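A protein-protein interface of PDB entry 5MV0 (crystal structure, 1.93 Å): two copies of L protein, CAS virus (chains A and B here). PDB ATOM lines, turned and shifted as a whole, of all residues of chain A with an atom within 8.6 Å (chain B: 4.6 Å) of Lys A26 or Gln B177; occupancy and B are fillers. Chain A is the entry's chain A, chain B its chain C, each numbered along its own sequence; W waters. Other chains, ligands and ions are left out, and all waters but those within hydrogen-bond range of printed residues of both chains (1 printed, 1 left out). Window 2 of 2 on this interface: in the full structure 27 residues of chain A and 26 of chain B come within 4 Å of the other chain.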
ATOM      1  N   LEU A  18     -29.345 -22.253 -15.210  1.00  0.00           N
ATOM      2  CA  LEU A  18     -28.453 -21.240 -14.655  1.00  0.00           C
ATOM      3  C   LEU A  18     -28.287 -20.056 -15.603  1.00  0.00           C
ATOM      4  O   LEU A  18     -28.003 -18.941 -15.149  1.00  0.00           O
ATOM      5  CB  LEU A  18     -27.090 -21.849 -14.315  1.00  0.00           C
ATOM      6  CG  LEU A  18     -27.099 -23.041 -13.349  1.00  0.00           C
ATOM      7  CD1 LEU A  18     -25.676 -23.519 -13.091  1.00  0.00           C
ATOM      8  CD2 LEU A  18     -27.788 -22.684 -12.051  1.00  0.00           C
ATOM      9  N   GLU A  21     -31.626 -18.135 -14.489  1.00  0.00           N
ATOM     10  CA  GLU A  21     -31.501 -17.563 -13.145  1.00  0.00           C
ATOM     11  C   GLU A  21     -30.052 -17.651 -12.677  1.00  0.00           C
ATOM     12  O   GLU A  21     -29.684 -18.584 -11.946  1.00  0.00           O
ATOM     13  CB  GLU A  21     -32.402 -18.266 -12.127  1.00  0.00           C
ATOM     14  CG  GLU A  21     -33.880 -18.029 -12.282  1.00  0.00           C
ATOM     15  CD  GLU A  21     -34.322 -16.638 -11.862  1.00  0.00           C
ATOM     16  OE1 GLU A  21     -35.500 -16.340 -12.086  1.00  0.00           O
ATOM     17  OE2 GLU A  21     -33.513 -15.843 -11.323  1.00  0.00           O
ATOM     18  N   PRO A  22     -29.212 -16.683 -13.058  1.00  0.00           N
ATOM     19  CA  PRO A  22     -27.790 -16.720 -12.658  1.00  0.00           C
ATOM     20  C   PRO A  22     -27.541 -16.761 -11.155  1.00  0.00           C
ATOM     21  O   PRO A  22     -26.490 -17.260 -10.729  1.00  0.00           O
ATOM     22  CB  PRO A  22     -27.227 -15.425 -13.265  1.00  0.00           C
ATOM     23  CG  PRO A  22     -28.136 -15.122 -14.423  1.00  0.00           C
ATOM     24  CD  PRO A  22     -29.497 -15.650 -14.072  1.00  0.00           C
ATOM     25  N   ASP A  23     -28.452 -16.231 -10.336  1.00  0.00           N
ATOM     26  CA  ASP A  23     -28.246 -16.297  -8.890  1.00  0.00           C
ATOM     27  C   ASP A  23     -28.126 -17.740  -8.409  1.00  0.00           C
ATOM     28  O   ASP A  23     -27.419 -18.015  -7.428  1.00  0.00           O
ATOM     29  CB  ASP A  23     -29.388 -15.590  -8.153  1.00  0.00           C
ATOM     30  CG  ASP A  23     -29.419 -14.082  -8.402  1.00  0.00           C
ATOM     31  OD1 ASP A  23     -28.347 -13.485  -8.661  1.00  0.00           O
ATOM     32  OD2 ASP A  23     -30.526 -13.494  -8.341  1.00  0.00           O
ATOM     33  N   LEU A  24     -28.787 -18.675  -9.100  1.00  0.00           N
ATOM     34  CA  LEU A  24     -28.698 -20.092  -8.751  1.00  0.00           C
ATOM     35  C   LEU A  24     -27.298 -20.664  -8.930  1.00  0.00           C
ATOM     36  O   LEU A  24     -26.988 -21.715  -8.350  1.00  0.00           O
ATOM     37  CB  LEU A  24     -29.676 -20.904  -9.604  1.00  0.00           C
ATOM     38  CG  LEU A  24     -31.142 -20.536  -9.373  1.00  0.00           C
ATOM     39  CD1 LEU A  24     -32.074 -21.311 -10.312  1.00  0.00           C
ATOM     40  CD2 LEU A  24     -31.445 -20.824  -7.937  1.00  0.00           C
ATOM     41  N   TYR A  25     -26.463 -20.022  -9.744  1.00  0.00           N
ATOM     42  CA  TYR A  25     -25.114 -20.533  -9.976  1.00  0.00           C
ATOM     43  C   TYR A  25     -24.341 -20.658  -8.671  1.00  0.00           C
ATOM     44  O   TYR A  25     -23.611 -21.634  -8.466  1.00  0.00           O
ATOM     45  CB  TYR A  25     -24.383 -19.621 -10.959  1.00  0.00           C
ATOM     46  CG  TYR A  25     -22.866 -19.734 -10.953  1.00  0.00           C
ATOM     47  CD1 TYR A  25     -22.080 -18.819 -10.251  1.00  0.00           C
ATOM     48  CD2 TYR A  25     -22.225 -20.735 -11.669  1.00  0.00           C
ATOM     49  CE1 TYR A  25     -20.699 -18.915 -10.247  1.00  0.00           C
ATOM     50  CE2 TYR A  25     -20.848 -20.842 -11.678  1.00  0.00           C
ATOM     51  CZ  TYR A  25     -20.085 -19.933 -10.969  1.00  0.00           C
ATOM     52  OH  TYR A  25     -18.707 -20.044 -10.991  1.00  0.00           O
ATOM     53  N   LYS A  26     -24.499 -19.687  -7.763  1.00  0.00           N
ATOM     54  CA  LYS A  26     -23.756 -19.744  -6.510  1.00  0.00           C
ATOM     55  C   LYS A  26     -24.171 -20.945  -5.673  1.00  0.00           C
ATOM     56  O   LYS A  26     -23.364 -21.474  -4.902  1.00  0.00           O
ATOM     57  CB  LYS A  26     -23.950 -18.452  -5.709  1.00  0.00           C
ATOM     58  CG  LYS A  26     -23.577 -17.182  -6.456  1.00  0.00           C
ATOM     59  CD  LYS A  26     -23.808 -15.939  -5.593  1.00  0.00           C
ATOM     60  CE  LYS A  26     -23.814 -14.653  -6.440  1.00  0.00           C
ATOM     61  NZ  LYS A  26     -22.962 -14.709  -7.672  1.00  0.00           N
ATOM     62  N   GLN A  27     -25.406 -21.412  -5.843  1.00  0.00           N
ATOM     63  CA  GLN A  27     -25.969 -22.452  -5.003  1.00  0.00           C
ATOM     64  C   GLN A  27     -25.880 -23.839  -5.618  1.00  0.00           C
ATOM     65  O   GLN A  27     -26.150 -24.825  -4.925  1.00  0.00           O
ATOM     66  CB  GLN A  27     -27.435 -22.136  -4.718  1.00  0.00           C
ATOM     67  CG  GLN A  27     -27.706 -20.662  -4.535  1.00  0.00           C
ATOM     68  CD  GLN A  27     -29.009 -20.410  -3.813  1.00  0.00           C
ATOM     69  OE1 GLN A  27     -29.906 -19.763  -4.355  1.00  0.00           O
ATOM     70  NE2 GLN A  27     -29.124 -20.917  -2.584  1.00  0.00           N
ATOM     71  N   SER A  28     -25.523 -23.946  -6.889  1.00  0.00           N
ATOM     72  CA  SER A  28     -25.664 -25.203  -7.587  1.00  0.00           C
ATOM     73  C   SER A  28     -24.306 -25.662  -8.089  1.00  0.00           C
ATOM     74  O   SER A  28     -23.293 -24.982  -7.937  1.00  0.00           O
ATOM     75  CB  SER A  28     -26.664 -25.073  -8.740  1.00  0.00           C
ATOM     76  OG  SER A  28     -27.027 -26.360  -9.218  1.00  0.00           O
ATOM     77  N   SER A  29     -24.294 -26.842  -8.689  1.00  0.00           N
ATOM     78  CA  SER A  29     -23.058 -27.399  -9.205  1.00  0.00           C
ATOM     79  C   SER A  29     -23.373 -28.176 -10.465  1.00  0.00           C
ATOM     80  O   SER A  29     -24.454 -28.759 -10.616  1.00  0.00           O
ATOM     81  CB  SER A  29     -22.369 -28.301  -8.182  1.00  0.00           C
ATOM     82  OG  SER A  29     -23.309 -29.176  -7.602  1.00  0.00           O
ATOM     83  N   LEU A  44     -31.185 -28.386  -6.597  1.00  0.00           N
ATOM     84  CA  LEU A  44     -31.544 -27.229  -7.422  1.00  0.00           C
ATOM     85  C   LEU A  44     -33.056 -27.087  -7.552  1.00  0.00           C
ATOM     86  O   LEU A  44     -33.590 -25.974  -7.550  1.00  0.00           O
ATOM     87  CB  LEU A  44     -30.905 -27.363  -8.804  1.00  0.00           C
ATOM     88  CG  LEU A  44     -31.160 -26.246  -9.832  1.00  0.00           C
ATOM     89  CD1 LEU A  44     -30.646 -24.910  -9.310  1.00  0.00           C
ATOM     90  CD2 LEU A  44     -30.503 -26.594 -11.169  1.00  0.00           C
ATOM     91  N   THR A  47     -34.187 -25.432  -4.532  1.00  0.00           N
ATOM     92  CA  THR A  47     -33.719 -24.048  -4.429  1.00  0.00           C
ATOM     93  C   THR A  47     -34.503 -23.119  -5.358  1.00  0.00           C
ATOM     94  O   THR A  47     -34.776 -21.964  -5.005  1.00  0.00           O
ATOM     95  CB  THR A  47     -32.221 -23.999  -4.731  1.00  0.00           C
ATOM     96  OG1 THR A  47     -31.549 -24.870  -3.816  1.00  0.00           O
ATOM     97  CG2 THR A  47     -31.675 -22.572  -4.565  1.00  0.00           C
ATOM     98  N   THR A  63     -29.637 -17.035   0.788  1.00  0.00           N
ATOM     99  CA  THR A  63     -28.598 -17.864   0.169  1.00  0.00           C
ATOM    100  C   THR A  63     -27.313 -17.933   0.977  1.00  0.00           C
ATOM    101  O   THR A  63     -26.544 -18.879   0.802  1.00  0.00           O
ATOM    102  CB  THR A  63     -28.245 -17.346  -1.229  1.00  0.00           C
ATOM    103  OG1 THR A  63     -27.847 -15.975  -1.132  1.00  0.00           O
ATOM    104  CG2 THR A  63     -29.424 -17.457  -2.157  1.00  0.00           C
ATOM    105  N   LYS A  64     -27.033 -16.950   1.826  1.00  0.00           N
ATOM    106  CA  LYS A  64     -25.863 -17.017   2.691  1.00  0.00           C
ATOM    107  C   LYS A  64     -26.147 -17.743   4.001  1.00  0.00           C
ATOM    108  O   LYS A  64     -25.262 -17.807   4.865  1.00  0.00           O
ATOM    109  CB  LYS A  64     -25.343 -15.606   2.967  1.00  0.00           C
ATOM    110  CG  LYS A  64     -24.999 -14.850   1.682  1.00  0.00           C
ATOM    111  CD  LYS A  64     -24.717 -13.390   1.996  1.00  0.00           C
ATOM    112  CE  LYS A  64     -25.115 -12.477   0.864  1.00  0.00           C
ATOM    113  NZ  LYS A  64     -24.878 -11.069   1.265  1.00  0.00           N
ATOM    114  N   LYS B  36     -16.527 -19.425  -5.591  1.00  0.00           N
ATOM    115  CA  LYS B  36     -17.239 -20.679  -5.387  1.00  0.00           C
ATOM    116  C   LYS B  36     -16.340 -21.715  -4.727  1.00  0.00           C
ATOM    117  O   LYS B  36     -16.760 -22.420  -3.799  1.00  0.00           O
ATOM    118  CB  LYS B  36     -17.764 -21.178  -6.730  1.00  0.00           C
ATOM    119  CG  LYS B  36     -18.822 -22.246  -6.616  1.00  0.00           C
ATOM    120  CD  LYS B  36     -19.570 -22.384  -7.941  1.00  0.00           C
ATOM    121  CE  LYS B  36     -20.757 -23.316  -7.794  1.00  0.00           C
ATOM    122  NZ  LYS B  36     -21.442 -23.506  -9.091  1.00  0.00           N
ATOM    123  N   LYS B 174     -16.343  -8.213  -3.753  1.00  0.00           N
ATOM    124  CA  LYS B 174     -17.053  -9.233  -4.521  1.00  0.00           C
ATOM    125  C   LYS B 174     -17.550 -10.337  -3.593  1.00  0.00           C
ATOM    126  O   LYS B 174     -18.613 -10.929  -3.813  1.00  0.00           O
ATOM    127  CB  LYS B 174     -16.114  -9.809  -5.592  1.00  0.00           C
ATOM    128  CG  LYS B 174     -16.754 -10.288  -6.890  1.00  0.00           C
ATOM    129  CD  LYS B 174     -17.678 -11.484  -6.695  1.00  0.00           C
ATOM    130  CE  LYS B 174     -18.133 -12.047  -8.040  1.00  0.00           C
ATOM    131  NZ  LYS B 174     -19.208 -13.085  -7.931  1.00  0.00           N
ATOM    132  N   SER B 175     -16.761 -10.614  -2.555  1.00  0.00           N
ATOM    133  CA  SER B 175     -17.084 -11.633  -1.569  1.00  0.00           C
ATOM    134  C   SER B 175     -18.439 -11.425  -0.924  1.00  0.00           C
ATOM    135  O   SER B 175     -19.034 -12.396  -0.445  1.00  0.00           O
ATOM    136  CB  SER B 175     -16.010 -11.653  -0.489  1.00  0.00           C
ATOM    137  OG  SER B 175     -14.728 -11.661  -1.078  1.00  0.00           O
ATOM    138  N   SER B 176     -18.937 -10.185  -0.887  1.00  0.00           N
ATOM    139  CA  SER B 176     -20.196  -9.920  -0.199  1.00  0.00           C
ATOM    140  C   SER B 176     -21.347 -10.700  -0.816  1.00  0.00           C
ATOM    141  O   SER B 176     -22.330 -10.995  -0.133  1.00  0.00           O
ATOM    142  CB  SER B 176     -20.509  -8.426  -0.227  1.00  0.00           C
ATOM    143  OG  SER B 176     -20.790  -8.012  -1.557  1.00  0.00           O
ATOM    144  N   GLN B 177     -21.258 -11.066  -2.058  1.00  0.00           N
ATOM    145  CA  GLN B 177     -22.317 -11.841  -2.643  1.00  0.00           C
ATOM    146  C   GLN B 177     -22.296 -13.297  -2.270  1.00  0.00           C
ATOM    147  O   GLN B 177     -23.230 -13.987  -2.529  1.00  0.00           O
ATOM    148  CB  GLN B 177     -22.192 -11.817  -4.147  1.00  0.00           C
ATOM    149  CG  GLN B 177     -22.299 -10.466  -4.783  1.00  0.00           C
ATOM    150  CD  GLN B 177     -21.968 -10.581  -6.238  1.00  0.00           C
ATOM    151  OE1 GLN B 177     -22.376 -11.536  -6.912  1.00  0.00           O
ATOM    152  NE2 GLN B 177     -21.189  -9.651  -6.732  1.00  0.00           N
ATOM    153  N   TRP B 178     -21.218 -13.739  -1.674  1.00  0.00           N
ATOM    154  CA  TRP B 178     -20.984 -15.156  -1.427  1.00  0.00           C
ATOM    155  C   TRP B 178     -21.067 -15.551   0.039  1.00  0.00           C
ATOM    156  O   TRP B 178     -21.272 -16.730   0.336  1.00  0.00           O
ATOM    157  CB  TRP B 178     -19.596 -15.556  -1.962  1.00  0.00           C
ATOM    158  CG  TRP B 178     -19.515 -15.536  -3.448  1.00  0.00           C
ATOM    159  CD1 TRP B 178     -19.197 -14.473  -4.246  1.00  0.00           C
ATOM    160  CD2 TRP B 178     -19.787 -16.635  -4.325  1.00  0.00           C
ATOM    161  NE1 TRP B 178     -19.247 -14.850  -5.569  1.00  0.00           N
ATOM    162  CE2 TRP B 178     -19.606 -16.172  -5.642  1.00  0.00           C
ATOM    163  CE3 TRP B 178     -20.165 -17.965  -4.122  1.00  0.00           C
ATOM    164  CZ2 TRP B 178     -19.783 -16.995  -6.752  1.00  0.00           C
ATOM    165  CZ3 TRP B 178     -20.344 -18.786  -5.237  1.00  0.00           C
ATOM    166  CH2 TRP B 178     -20.150 -18.296  -6.525  1.00  0.00           C
ATOM    167  N   ILE B 179     -20.898 -14.614   0.959  1.00  0.00           N
ATOM    168  CA  ILE B 179     -20.754 -14.957   2.366  1.00  0.00           C
ATOM    169  C   ILE B 179     -21.295 -13.791   3.173  1.00  0.00           C
ATOM    170  O   ILE B 179     -21.173 -12.629   2.767  1.00  0.00           O
ATOM    171  CB  ILE B 179     -19.279 -15.273   2.717  1.00  0.00           C
ATOM    172  CG1 ILE B 179     -19.159 -15.830   4.141  1.00  0.00           C
ATOM    173  CG2 ILE B 179     -18.395 -14.024   2.524  1.00  0.00           C
ATOM    174  CD1 ILE B 179     -17.800 -16.388   4.469  1.00  0.00           C
HETATM  175  O   HOH W   1     -24.786 -16.437  -1.530  1.00  0.00           O
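Of the 14 printed residues of chain A, 4 touch a printed residue of chain B. Printed residues of chain A that touch a printed residue of chain B: Tyr A25, Lys A26, Ser A28 and Lys A64. Hydrophobic or aromatic side chains of chain A within 4 Å of the printed part of chain B: Tyr A25. Hydrophobic or aromatic side chains of chain B that line the printed part of chain A: Trp B178. Among the printed residues, 7 pairs touch across the chains.
OE1 of Gln B177 is in hydrogen-bond range of NZ of Lys A26, at 3.3 Å. The side-chain amino group (NZ) of Lys B36 sits at hydrogen-bond distance from the backbone carbonyl oxygen (O) of Ser A28 (2.6 Å). O of Ser B176 is in hydrogen-bond range of NZ of Lys A64. The backbone carbonyl oxygen of Tyr A25 is in hydrogen-bond range of the side-chain amino group of Lys B36 (2.9 Å).
Of the printed residues of chain B, Tyr A25 touches Lys B36 (2.9 Å) and Trp B178 (3.8 Å). Of chain B, only Gln B177 and Trp B178 come within 4 Å of Lys A26. Of the printed residues of chain B, Ser A28 touches Lys B36 (2.6 Å). Of the printed residues of chain A, Lys B36 touches Tyr A25 (2.9 Å) and Ser A28 (2.6 Å). Ser B176 touches just one residue of chain A: Lys A64. Gln B177 touches just one residue of chain A: Lys A26. Of chain A, only Tyr A25 and Lys A26 come within 4 Å of Trp B178. The nearest residue of chain B that does not touch Lys A26 is Lys B174 (4.1 Å). The nearest printed residue of chain B that does not touch Tyr A25 is Lys B174 (6.4 Å).
No position is printed for both chains.
Water W1 bridges O of Gln B177 (3.1 Å) and OG1 of Thr A63 (3.1 Å).
Tyr A25 touches Trp B178 (CE1 to CH2, 3.8 Å). CH2 of Trp B178 touches CG of Lys A26 (3.6 Å). Lys A64 touches Ile B179 (CD to C, 3.6 Å).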
